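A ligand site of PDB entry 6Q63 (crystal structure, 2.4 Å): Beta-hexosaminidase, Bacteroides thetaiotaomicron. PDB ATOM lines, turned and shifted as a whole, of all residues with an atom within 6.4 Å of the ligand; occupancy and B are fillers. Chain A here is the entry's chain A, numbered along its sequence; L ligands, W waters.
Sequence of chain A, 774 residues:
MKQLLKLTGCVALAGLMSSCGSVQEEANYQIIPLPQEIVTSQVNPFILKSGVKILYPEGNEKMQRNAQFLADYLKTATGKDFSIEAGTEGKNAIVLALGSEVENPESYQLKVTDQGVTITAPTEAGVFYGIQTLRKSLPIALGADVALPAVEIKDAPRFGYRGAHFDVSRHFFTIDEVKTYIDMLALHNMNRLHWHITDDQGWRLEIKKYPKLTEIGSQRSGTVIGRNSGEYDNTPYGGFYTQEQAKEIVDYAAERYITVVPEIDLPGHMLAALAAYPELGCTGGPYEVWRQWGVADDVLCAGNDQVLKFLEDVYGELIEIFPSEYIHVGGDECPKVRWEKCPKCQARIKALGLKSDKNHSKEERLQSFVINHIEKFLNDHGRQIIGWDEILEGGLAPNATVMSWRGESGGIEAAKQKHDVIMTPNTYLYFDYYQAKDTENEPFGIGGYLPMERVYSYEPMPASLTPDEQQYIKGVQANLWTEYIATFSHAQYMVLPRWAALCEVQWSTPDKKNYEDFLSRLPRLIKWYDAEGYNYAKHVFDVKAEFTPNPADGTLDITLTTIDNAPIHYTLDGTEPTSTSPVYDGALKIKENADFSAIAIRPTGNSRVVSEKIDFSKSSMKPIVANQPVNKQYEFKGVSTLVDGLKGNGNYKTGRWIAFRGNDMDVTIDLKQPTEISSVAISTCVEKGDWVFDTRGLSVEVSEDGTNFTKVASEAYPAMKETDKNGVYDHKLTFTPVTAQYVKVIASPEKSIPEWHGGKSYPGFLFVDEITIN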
ATOM      1  N   ASP A 167     -31.569   1.016 -10.346  1.00  0.00           N
ATOM      2  CA  ASP A 167     -30.212   0.839 -10.911  1.00  0.00           C
ATOM      3  C   ASP A 167     -29.961   1.973 -11.912  1.00  0.00           C
ATOM      4  O   ASP A 167     -30.620   1.956 -12.965  1.00  0.00           O
ATOM      5  CB  ASP A 167     -30.076  -0.555 -11.551  1.00  0.00           C
ATOM      6  CG  ASP A 167     -28.804  -0.818 -12.316  1.00  0.00           C
ATOM      7  OD1 ASP A 167     -27.887   0.039 -12.292  1.00  0.00           O
ATOM      8  OD2 ASP A 167     -28.719  -1.903 -12.936  1.00  0.00           O
ATOM      9  N   ARG A 170     -26.142   0.700 -14.781  1.00  0.00           N
ATOM     10  CA  ARG A 170     -26.232  -0.096 -16.031  1.00  0.00           C
ATOM     11  C   ARG A 170     -26.699   0.819 -17.181  1.00  0.00           C
ATOM     12  O   ARG A 170     -26.058   0.811 -18.235  1.00  0.00           O
ATOM     13  CB  ARG A 170     -27.150  -1.298 -15.827  1.00  0.00           C
ATOM     14  CG  ARG A 170     -26.471  -2.507 -15.192  1.00  0.00           C
ATOM     15  CD  ARG A 170     -25.605  -2.198 -13.983  1.00  0.00           C
ATOM     16  NE  ARG A 170     -24.932  -3.409 -13.508  1.00  0.00           N
ATOM     17  CZ  ARG A 170     -25.490  -4.345 -12.754  1.00  0.00           C
ATOM     18  NH1 ARG A 170     -26.740  -4.242 -12.350  1.00  0.00           N
ATOM     19  NH2 ARG A 170     -24.776  -5.410 -12.411  1.00  0.00           N
ATOM     20  N   HIS A 196     -29.127   2.625  -6.303  1.00  0.00           N
ATOM     21  CA  HIS A 196     -27.961   1.800  -6.692  1.00  0.00           C
ATOM     22  C   HIS A 196     -27.112   2.588  -7.701  1.00  0.00           C
ATOM     23  O   HIS A 196     -27.399   2.497  -8.904  1.00  0.00           O
ATOM     24  CB  HIS A 196     -28.430   0.444  -7.244  1.00  0.00           C
ATOM     25  CG  HIS A 196     -27.326  -0.512  -7.545  1.00  0.00           C
ATOM     26  ND1 HIS A 196     -26.881  -1.445  -6.624  1.00  0.00           N
ATOM     27  CD2 HIS A 196     -26.585  -0.690  -8.663  1.00  0.00           C
ATOM     28  CE1 HIS A 196     -25.912  -2.147  -7.165  1.00  0.00           C
ATOM     29  NE2 HIS A 196     -25.704  -1.710  -8.409  1.00  0.00           N
ATOM     30  N   ASP A 199     -21.670   0.462 -10.092  1.00  0.00           N
ATOM     31  CA  ASP A 199     -21.526  -0.944 -10.518  1.00  0.00           C
ATOM     32  C   ASP A 199     -20.364  -1.030 -11.516  1.00  0.00           C
ATOM     33  O   ASP A 199     -19.619  -0.052 -11.646  1.00  0.00           O
ATOM     34  CB  ASP A 199     -22.840  -1.486 -11.077  1.00  0.00           C
ATOM     35  CG  ASP A 199     -23.104  -2.931 -10.708  1.00  0.00           C
ATOM     36  OD1 ASP A 199     -22.427  -3.816 -11.277  1.00  0.00           O
ATOM     37  OD2 ASP A 199     -23.975  -3.151  -9.834  1.00  0.00           O
ATOM     38  N   ASP A 265     -21.983  -0.573  -3.828  1.00  0.00           N
ATOM     39  CA  ASP A 265     -21.831  -2.048  -3.767  1.00  0.00           C
ATOM     40  C   ASP A 265     -20.345  -2.397  -3.614  1.00  0.00           C
ATOM     41  O   ASP A 265     -19.548  -1.935  -4.459  1.00  0.00           O
ATOM     42  CB  ASP A 265     -22.427  -2.686  -5.017  1.00  0.00           C
ATOM     43  CG  ASP A 265     -22.768  -4.160  -4.890  1.00  0.00           C
ATOM     44  OD1 ASP A 265     -22.187  -4.832  -4.001  1.00  0.00           O
ATOM     45  OD2 ASP A 265     -23.619  -4.621  -5.670  1.00  0.00           O
ATOM     46  N   HIS A 269     -18.768  -5.831  -7.921  1.00  0.00           N
ATOM     47  CA  HIS A 269     -19.506  -4.799  -8.697  1.00  0.00           C
ATOM     48  C   HIS A 269     -18.731  -3.472  -8.609  1.00  0.00           C
ATOM     49  O   HIS A 269     -19.376  -2.424  -8.418  1.00  0.00           O
ATOM     50  CB  HIS A 269     -20.957  -4.717  -8.202  1.00  0.00           C
ATOM     51  CG  HIS A 269     -21.763  -5.904  -8.611  1.00  0.00           C
ATOM     52  ND1 HIS A 269     -22.273  -6.041  -9.896  1.00  0.00           N
ATOM     53  CD2 HIS A 269     -22.134  -7.012  -7.939  1.00  0.00           C
ATOM     54  CE1 HIS A 269     -22.927  -7.182  -9.988  1.00  0.00           C
ATOM     55  NE2 HIS A 269     -22.857  -7.798  -8.805  1.00  0.00           N
ATOM     56  N   GLY A 294     -23.591  -8.977 -16.421  1.00  0.00           N
ATOM     57  CA  GLY A 294     -23.297 -10.191 -15.645  1.00  0.00           C
ATOM     58  C   GLY A 294     -22.424  -9.908 -14.449  1.00  0.00           C
ATOM     59  O   GLY A 294     -22.550  -8.808 -13.862  1.00  0.00           O
ATOM     60  N   VAL A 295     -21.547 -10.857 -14.109  1.00  0.00           N
ATOM     61  CA  VAL A 295     -20.744 -10.879 -12.848  1.00  0.00           C
ATOM     62  C   VAL A 295     -19.263 -10.846 -13.234  1.00  0.00           C
ATOM     63  O   VAL A 295     -18.837 -11.744 -13.989  1.00  0.00           O
ATOM     64  CB  VAL A 295     -21.114 -12.120 -12.003  1.00  0.00           C
ATOM     65  CG1 VAL A 295     -20.300 -12.206 -10.724  1.00  0.00           C
ATOM     66  CG2 VAL A 295     -22.597 -12.159 -11.700  1.00  0.00           C
ATOM     67  N   ASP A 332     -23.259  -8.513  -2.932  1.00  0.00           N
ATOM     68  CA  ASP A 332     -23.799  -9.516  -3.883  1.00  0.00           C
ATOM     69  C   ASP A 332     -22.707  -9.926  -4.871  1.00  0.00           C
ATOM     70  O   ASP A 332     -21.807  -9.114  -5.136  1.00  0.00           O
ATOM     71  CB  ASP A 332     -25.027  -8.995  -4.651  1.00  0.00           C
ATOM     72  CG  ASP A 332     -24.767  -7.750  -5.476  1.00  0.00           C
ATOM     73  OD1 ASP A 332     -23.992  -6.895  -5.020  1.00  0.00           O
ATOM     74  OD2 ASP A 332     -25.339  -7.645  -6.586  1.00  0.00           O
ATOM     75  N   GLU A 333     -22.782 -11.175  -5.367  1.00  0.00           N
ATOM     76  CA  GLU A 333     -22.036 -11.674  -6.556  1.00  0.00           C
ATOM     77  C   GLU A 333     -20.597 -11.172  -6.541  1.00  0.00           C
ATOM     78  O   GLU A 333     -20.198 -10.466  -7.500  1.00  0.00           O
ATOM     79  CB  GLU A 333     -22.751 -11.216  -7.831  1.00  0.00           C
ATOM     80  CG  GLU A 333     -24.131 -11.833  -7.998  1.00  0.00           C
ATOM     81  CD  GLU A 333     -24.907 -11.275  -9.184  1.00  0.00           C
ATOM     82  OE1 GLU A 333     -24.621 -10.133  -9.580  1.00  0.00           O
ATOM     83  OE2 GLU A 333     -25.774 -12.004  -9.714  1.00  0.00           O
ATOM     84  N   TRP A 388     -26.949  -7.408   0.762  1.00  0.00           N
ATOM     85  CA  TRP A 388     -27.594  -8.527   0.030  1.00  0.00           C
ATOM     86  C   TRP A 388     -27.299  -9.829   0.797  1.00  0.00           C
ATOM     87  O   TRP A 388     -26.308  -9.863   1.540  1.00  0.00           O
ATOM     88  CB  TRP A 388     -27.108  -8.587  -1.424  1.00  0.00           C
ATOM     89  CG  TRP A 388     -27.393  -7.358  -2.222  1.00  0.00           C
ATOM     90  CD1 TRP A 388     -26.484  -6.463  -2.695  1.00  0.00           C
ATOM     91  CD2 TRP A 388     -28.686  -6.883  -2.658  1.00  0.00           C
ATOM     92  NE1 TRP A 388     -27.104  -5.467  -3.402  1.00  0.00           N
ATOM     93  CE2 TRP A 388     -28.454  -5.689  -3.394  1.00  0.00           C
ATOM     94  CE3 TRP A 388     -30.001  -7.330  -2.503  1.00  0.00           C
ATOM     95  CZ2 TRP A 388     -29.494  -4.959  -3.967  1.00  0.00           C
ATOM     96  CZ3 TRP A 388     -31.026  -6.608  -3.075  1.00  0.00           C
ATOM     97  CH2 TRP A 388     -30.776  -5.441  -3.794  1.00  0.00           C
ATOM     98  N   GLU A 390     -25.907 -12.521   0.372  1.00  0.00           N
ATOM     99  CA  GLU A 390     -24.533 -13.080   0.282  1.00  0.00           C
ATOM    100  C   GLU A 390     -23.690 -12.689   1.497  1.00  0.00           C
ATOM    101  O   GLU A 390     -22.681 -13.382   1.747  1.00  0.00           O
ATOM    102  CB  GLU A 390     -23.807 -12.628  -1.000  1.00  0.00           C
ATOM    103  CG  GLU A 390     -24.303 -13.316  -2.257  1.00  0.00           C
ATOM    104  CD  GLU A 390     -25.283 -12.484  -3.069  1.00  0.00           C
ATOM    105  OE1 GLU A 390     -26.117 -11.796  -2.447  1.00  0.00           O
ATOM    106  OE2 GLU A 390     -25.181 -12.510  -4.322  1.00  0.00           O
ATOM    107  N   TRP A 405     -32.724 -11.577  -1.765  1.00  0.00           N
ATOM    108  CA  TRP A 405     -33.036 -11.453  -3.207  1.00  0.00           C
ATOM    109  C   TRP A 405     -32.957 -12.818  -3.914  1.00  0.00           C
ATOM    110  O   TRP A 405     -33.783 -13.023  -4.824  1.00  0.00           O
ATOM    111  CB  TRP A 405     -32.136 -10.404  -3.878  1.00  0.00           C
ATOM    112  CG  TRP A 405     -30.743 -10.846  -4.169  1.00  0.00           C
ATOM    113  CD1 TRP A 405     -29.660 -10.737  -3.337  1.00  0.00           C
ATOM    114  CD2 TRP A 405     -30.250 -11.437  -5.385  1.00  0.00           C
ATOM    115  NE1 TRP A 405     -28.542 -11.235  -3.948  1.00  0.00           N
ATOM    116  CE2 TRP A 405     -28.867 -11.666  -5.208  1.00  0.00           C
ATOM    117  CE3 TRP A 405     -30.840 -11.805  -6.598  1.00  0.00           C
ATOM    118  CZ2 TRP A 405     -28.077 -12.249  -6.204  1.00  0.00           C
ATOM    119  CZ3 TRP A 405     -30.064 -12.374  -7.582  1.00  0.00           C
ATOM    120  CH2 TRP A 405     -28.699 -12.597  -7.383  1.00  0.00           C
ATOM    121  N   TYR A 430     -38.584  -8.865  -8.709  1.00  0.00           N
ATOM    122  CA  TYR A 430     -37.552  -8.411  -9.682  1.00  0.00           C
ATOM    123  C   TYR A 430     -38.250  -7.906 -10.949  1.00  0.00           C
ATOM    124  O   TYR A 430     -38.553  -8.716 -11.854  1.00  0.00           O
ATOM    125  CB  TYR A 430     -36.520  -9.527  -9.935  1.00  0.00           C
ATOM    126  CG  TYR A 430     -35.276  -9.395  -9.104  1.00  0.00           C
ATOM    127  CD1 TYR A 430     -35.331  -9.095  -7.751  1.00  0.00           C
ATOM    128  CD2 TYR A 430     -34.014  -9.566  -9.667  1.00  0.00           C
ATOM    129  CE1 TYR A 430     -34.193  -8.951  -6.981  1.00  0.00           C
ATOM    130  CE2 TYR A 430     -32.862  -9.435  -8.908  1.00  0.00           C
ATOM    131  CZ  TYR A 430     -32.947  -9.119  -7.558  1.00  0.00           C
ATOM    132  OH  TYR A 430     -31.818  -8.969  -6.805  1.00  0.00           O
ATOM    133  N   ASP A 432     -37.360  -6.098 -13.472  1.00  0.00           N
ATOM    134  CA  ASP A 432     -36.647  -6.146 -14.775  1.00  0.00           C
ATOM    135  C   ASP A 432     -37.125  -7.391 -15.552  1.00  0.00           C
ATOM    136  O   ASP A 432     -36.921  -7.416 -16.773  1.00  0.00           O
ATOM    137  CB  ASP A 432     -35.119  -6.119 -14.612  1.00  0.00           C
ATOM    138  CG  ASP A 432     -34.563  -7.096 -13.587  1.00  0.00           C
ATOM    139  OD1 ASP A 432     -35.144  -7.194 -12.495  1.00  0.00           O
ATOM    140  OD2 ASP A 432     -33.546  -7.754 -13.889  1.00  0.00           O
ATOM    141  N   TYR A 433     -37.741  -8.353 -14.872  1.00  0.00           N
ATOM    142  CA  TYR A 433     -38.300  -9.601 -15.481  1.00  0.00           C
ATOM    143  C   TYR A 433     -39.556  -9.259 -16.299  1.00  0.00           C
ATOM    144  O   TYR A 433     -40.313  -8.344 -15.903  1.00  0.00           O
ATOM    145  CB  TYR A 433     -38.624 -10.651 -14.414  1.00  0.00           C
ATOM    146  CG  TYR A 433     -37.443 -11.203 -13.658  1.00  0.00           C
ATOM    147  CD1 TYR A 433     -36.140 -10.828 -13.950  1.00  0.00           C
ATOM    148  CD2 TYR A 433     -37.628 -12.142 -12.642  1.00  0.00           C
ATOM    149  CE1 TYR A 433     -35.063 -11.352 -13.262  1.00  0.00           C
ATOM    150  CE2 TYR A 433     -36.558 -12.664 -11.939  1.00  0.00           C
ATOM    151  CZ  TYR A 433     -35.270 -12.271 -12.252  1.00  0.00           C
ATOM    152  OH  TYR A 433     -34.210 -12.779 -11.561  1.00  0.00           O
ATOM    153  N   ILE A 446     -34.338  -9.105 -19.690  1.00  0.00           N
ATOM    154  CA  ILE A 446     -33.364 -10.114 -19.173  1.00  0.00           C
ATOM    155  C   ILE A 446     -33.959 -11.528 -19.286  1.00  0.00           C
ATOM    156  O   ILE A 446     -33.187 -12.460 -19.591  1.00  0.00           O
ATOM    157  CB  ILE A 446     -32.917  -9.797 -17.732  1.00  0.00           C
ATOM    158  CG1 ILE A 446     -31.887 -10.815 -17.235  1.00  0.00           C
ATOM    159  CG2 ILE A 446     -34.112  -9.697 -16.783  1.00  0.00           C
ATOM    160  CD1 ILE A 446     -31.060 -10.347 -16.066  1.00  0.00           C
ATOM    161  N   ASN A 479     -37.048  -4.464  -7.006  1.00  0.00           N
ATOM    162  CA  ASN A 479     -35.787  -3.955  -7.592  1.00  0.00           C
ATOM    163  C   ASN A 479     -35.998  -3.746  -9.099  1.00  0.00           C
ATOM    164  O   ASN A 479     -36.732  -4.548  -9.708  1.00  0.00           O
ATOM    165  CB  ASN A 479     -34.610  -4.882  -7.286  1.00  0.00           C
ATOM    166  CG  ASN A 479     -34.398  -5.080  -5.799  1.00  0.00           C
ATOM    167  OD1 ASN A 479     -34.835  -4.271  -4.989  1.00  0.00           O
ATOM    168  ND2 ASN A 479     -33.726  -6.159  -5.429  1.00  0.00           N
ATOM    169  N   TRP A 481     -33.323  -3.438 -12.019  1.00  0.00           N
ATOM    170  CA  TRP A 481     -31.999  -3.492 -12.687  1.00  0.00           C
ATOM    171  C   TRP A 481     -32.208  -3.068 -14.141  1.00  0.00           C
ATOM    172  O   TRP A 481     -33.266  -3.412 -14.695  1.00  0.00           O
ATOM    173  CB  TRP A 481     -31.388  -4.881 -12.540  1.00  0.00           C
ATOM    174  CG  TRP A 481     -31.362  -5.352 -11.119  1.00  0.00           C
ATOM    175  CD1 TRP A 481     -32.274  -6.166 -10.509  1.00  0.00           C
ATOM    176  CD2 TRP A 481     -30.402  -4.995 -10.114  1.00  0.00           C
ATOM    177  NE1 TRP A 481     -31.927  -6.357  -9.192  1.00  0.00           N
ATOM    178  CE2 TRP A 481     -30.784  -5.641  -8.919  1.00  0.00           C
ATOM    179  CE3 TRP A 481     -29.243  -4.201 -10.103  1.00  0.00           C
ATOM    180  CZ2 TRP A 481     -30.056  -5.530  -7.737  1.00  0.00           C
ATOM    181  CZ3 TRP A 481     -28.523  -4.084  -8.938  1.00  0.00           C
ATOM    182  CH2 TRP A 481     -28.931  -4.746  -7.772  1.00  0.00           C
ATOM    183  N   THR A 482     -31.266  -2.328 -14.722  1.00  0.00           N
ATOM    184  CA  THR A 482     -31.496  -1.552 -15.968  1.00  0.00           C
ATOM    185  C   THR A 482     -30.507  -1.944 -17.073  1.00  0.00           C
ATOM    186  O   THR A 482     -30.247  -1.085 -17.932  1.00  0.00           O
ATOM    187  CB  THR A 482     -31.437  -0.050 -15.665  1.00  0.00           C
ATOM    188  OG1 THR A 482     -30.189   0.236 -15.026  1.00  0.00           O
ATOM    189  CG2 THR A 482     -32.591   0.411 -14.793  1.00  0.00           C
ATOM    190  N   GLU A 483     -30.039  -3.194 -17.099  1.00  0.00           N
ATOM    191  CA  GLU A 483     -29.213  -3.717 -18.218  1.00  0.00           C
ATOM    192  C   GLU A 483     -29.967  -3.496 -19.549  1.00  0.00           C
ATOM    193  O   GLU A 483     -29.297  -3.168 -20.543  1.00  0.00           O
ATOM    194  CB  GLU A 483     -28.883  -5.206 -18.051  1.00  0.00           C
ATOM    195  CG  GLU A 483     -27.927  -5.507 -16.907  1.00  0.00           C
ATOM    196  CD  GLU A 483     -28.587  -5.939 -15.605  1.00  0.00           C
ATOM    197  OE1 GLU A 483     -29.700  -5.461 -15.320  1.00  0.00           O
ATOM    198  OE2 GLU A 483     -27.985  -6.767 -14.899  1.00  0.00           O
HETATM  199  C1  LIG L   1     -28.008 -10.048 -10.137  1.00  0.00           C
HETATM  200  C2  LIG L   1     -27.264  -8.806  -9.597  1.00  0.00           C
HETATM  201  C3  LIG L   1     -27.682  -7.524 -10.346  1.00  0.00           C
HETATM  202  C4  LIG L   1     -28.411  -7.875 -11.649  1.00  0.00           C
HETATM  203  C5  LIG L   1     -29.664  -8.707 -11.335  1.00  0.00           C
HETATM  204  C6  LIG L   1     -30.314  -9.243 -12.615  1.00  0.00           C
HETATM  205  C7  LIG L   1     -28.430  -8.763  -7.383  1.00  0.00           C
HETATM  206  C8  LIG L   1     -28.253  -8.512  -5.916  1.00  0.00           C
HETATM  207  N1  LIG L   1     -27.328  -8.657  -8.130  1.00  0.00           N
HETATM  208  O1  LIG L   1     -27.329 -10.533 -11.300  1.00  0.00           O
HETATM  209  O2  LIG L   1     -26.520  -6.733 -10.606  1.00  0.00           O
HETATM  210  O3  LIG L   1     -28.774  -6.682 -12.351  1.00  0.00           O
HETATM  211  O4  LIG L   1     -29.387  -9.792 -10.435  1.00  0.00           O
HETATM  212  O5  LIG L   1     -31.751  -9.171 -12.506  1.00  0.00           O
HETATM  213  O6  LIG L   1     -29.524  -9.046  -7.827  1.00  0.00           O
HETATM  214  O   HOH W   1     -25.306  -5.344  -8.546  1.00  0.00           O
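OH of Tyr 430 is in hydrogen-bond range of O6 of the ligand (2.5 Å).
O1 of the ligand sits at hydrogen-bond distance from OE2 of Glu 333.
The side-chain carboxylate (OE2) of Glu 483 sits at hydrogen-bond distance from an oxygen (O3) of the ligand, 2.7 Å away.
The side-chain carboxylate (OD2) of Asp 432 is in hydrogen-bond range of an oxygen (O5) of the ligand.
OD2 of Asp 332 sits at hydrogen-bond distance from N1 of the ligand, 2.7 Å away.
O2 of the ligand is in hydrogen-bond range of NH2 of Arg 170 (2.8 Å).
NE2 of His 269 is in hydrogen-bond range of OE1 of Glu 333.
The backbone NH of Glu 333 is in hydrogen-bond range of the side-chain carboxylate of Glu 390 (2.9 Å).
OE2 of Glu 483 is in salt-bridge range of NH1 of Arg 170, 3.8 Å away.
The side-chain carboxylate (OD2) of Asp 332 is in hydrogen-bond range of a ring nitrogen (NE2) of His 269, 3.3 Å away.
The side-chain carboxylate (OD1) of Asp 199 lies within salt-bridge range of the guanidinium group (NH2) of Arg 170, 3.1 Å away.
The guanidinium group of Arg 170 lies within salt-bridge range of the side-chain carboxylate of Asp 167 (3.1 Å).
NE1 of Trp 405 sits at hydrogen-bond distance from OE1 of Glu 390 (2.9 Å).
The side-chain carboxylate of Asp 199 sits at hydrogen-bond distance from a ring nitrogen (ND1) of His 269 (2.6 Å).
CE1 of His 269 touches O2 of the ligand, at 3.7 Å.
Trp 388 touches the ligand.
CE2 of Trp 405 touches C8 of the ligand, at 3.3 Å.
Ile 446 touches the ligand.
Trp 481 touches the ligand (CG to O3, 3.2 Å).
Hydrophobic or aromatic side chains that line the ligand: His 269, Trp 388, Trp 405, Tyr 430, Ile 446 and Trp 481.
Within 4 Å of the ligand: Arg 170, His 269, Asp 332, Glu 333, Trp 388, Trp 405, Tyr 430, Asp 432, Ile 446, Trp 481 and Glu 483.
The nearest printed residue that does not touch the ligand is Tyr 433 (4.04 Å).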
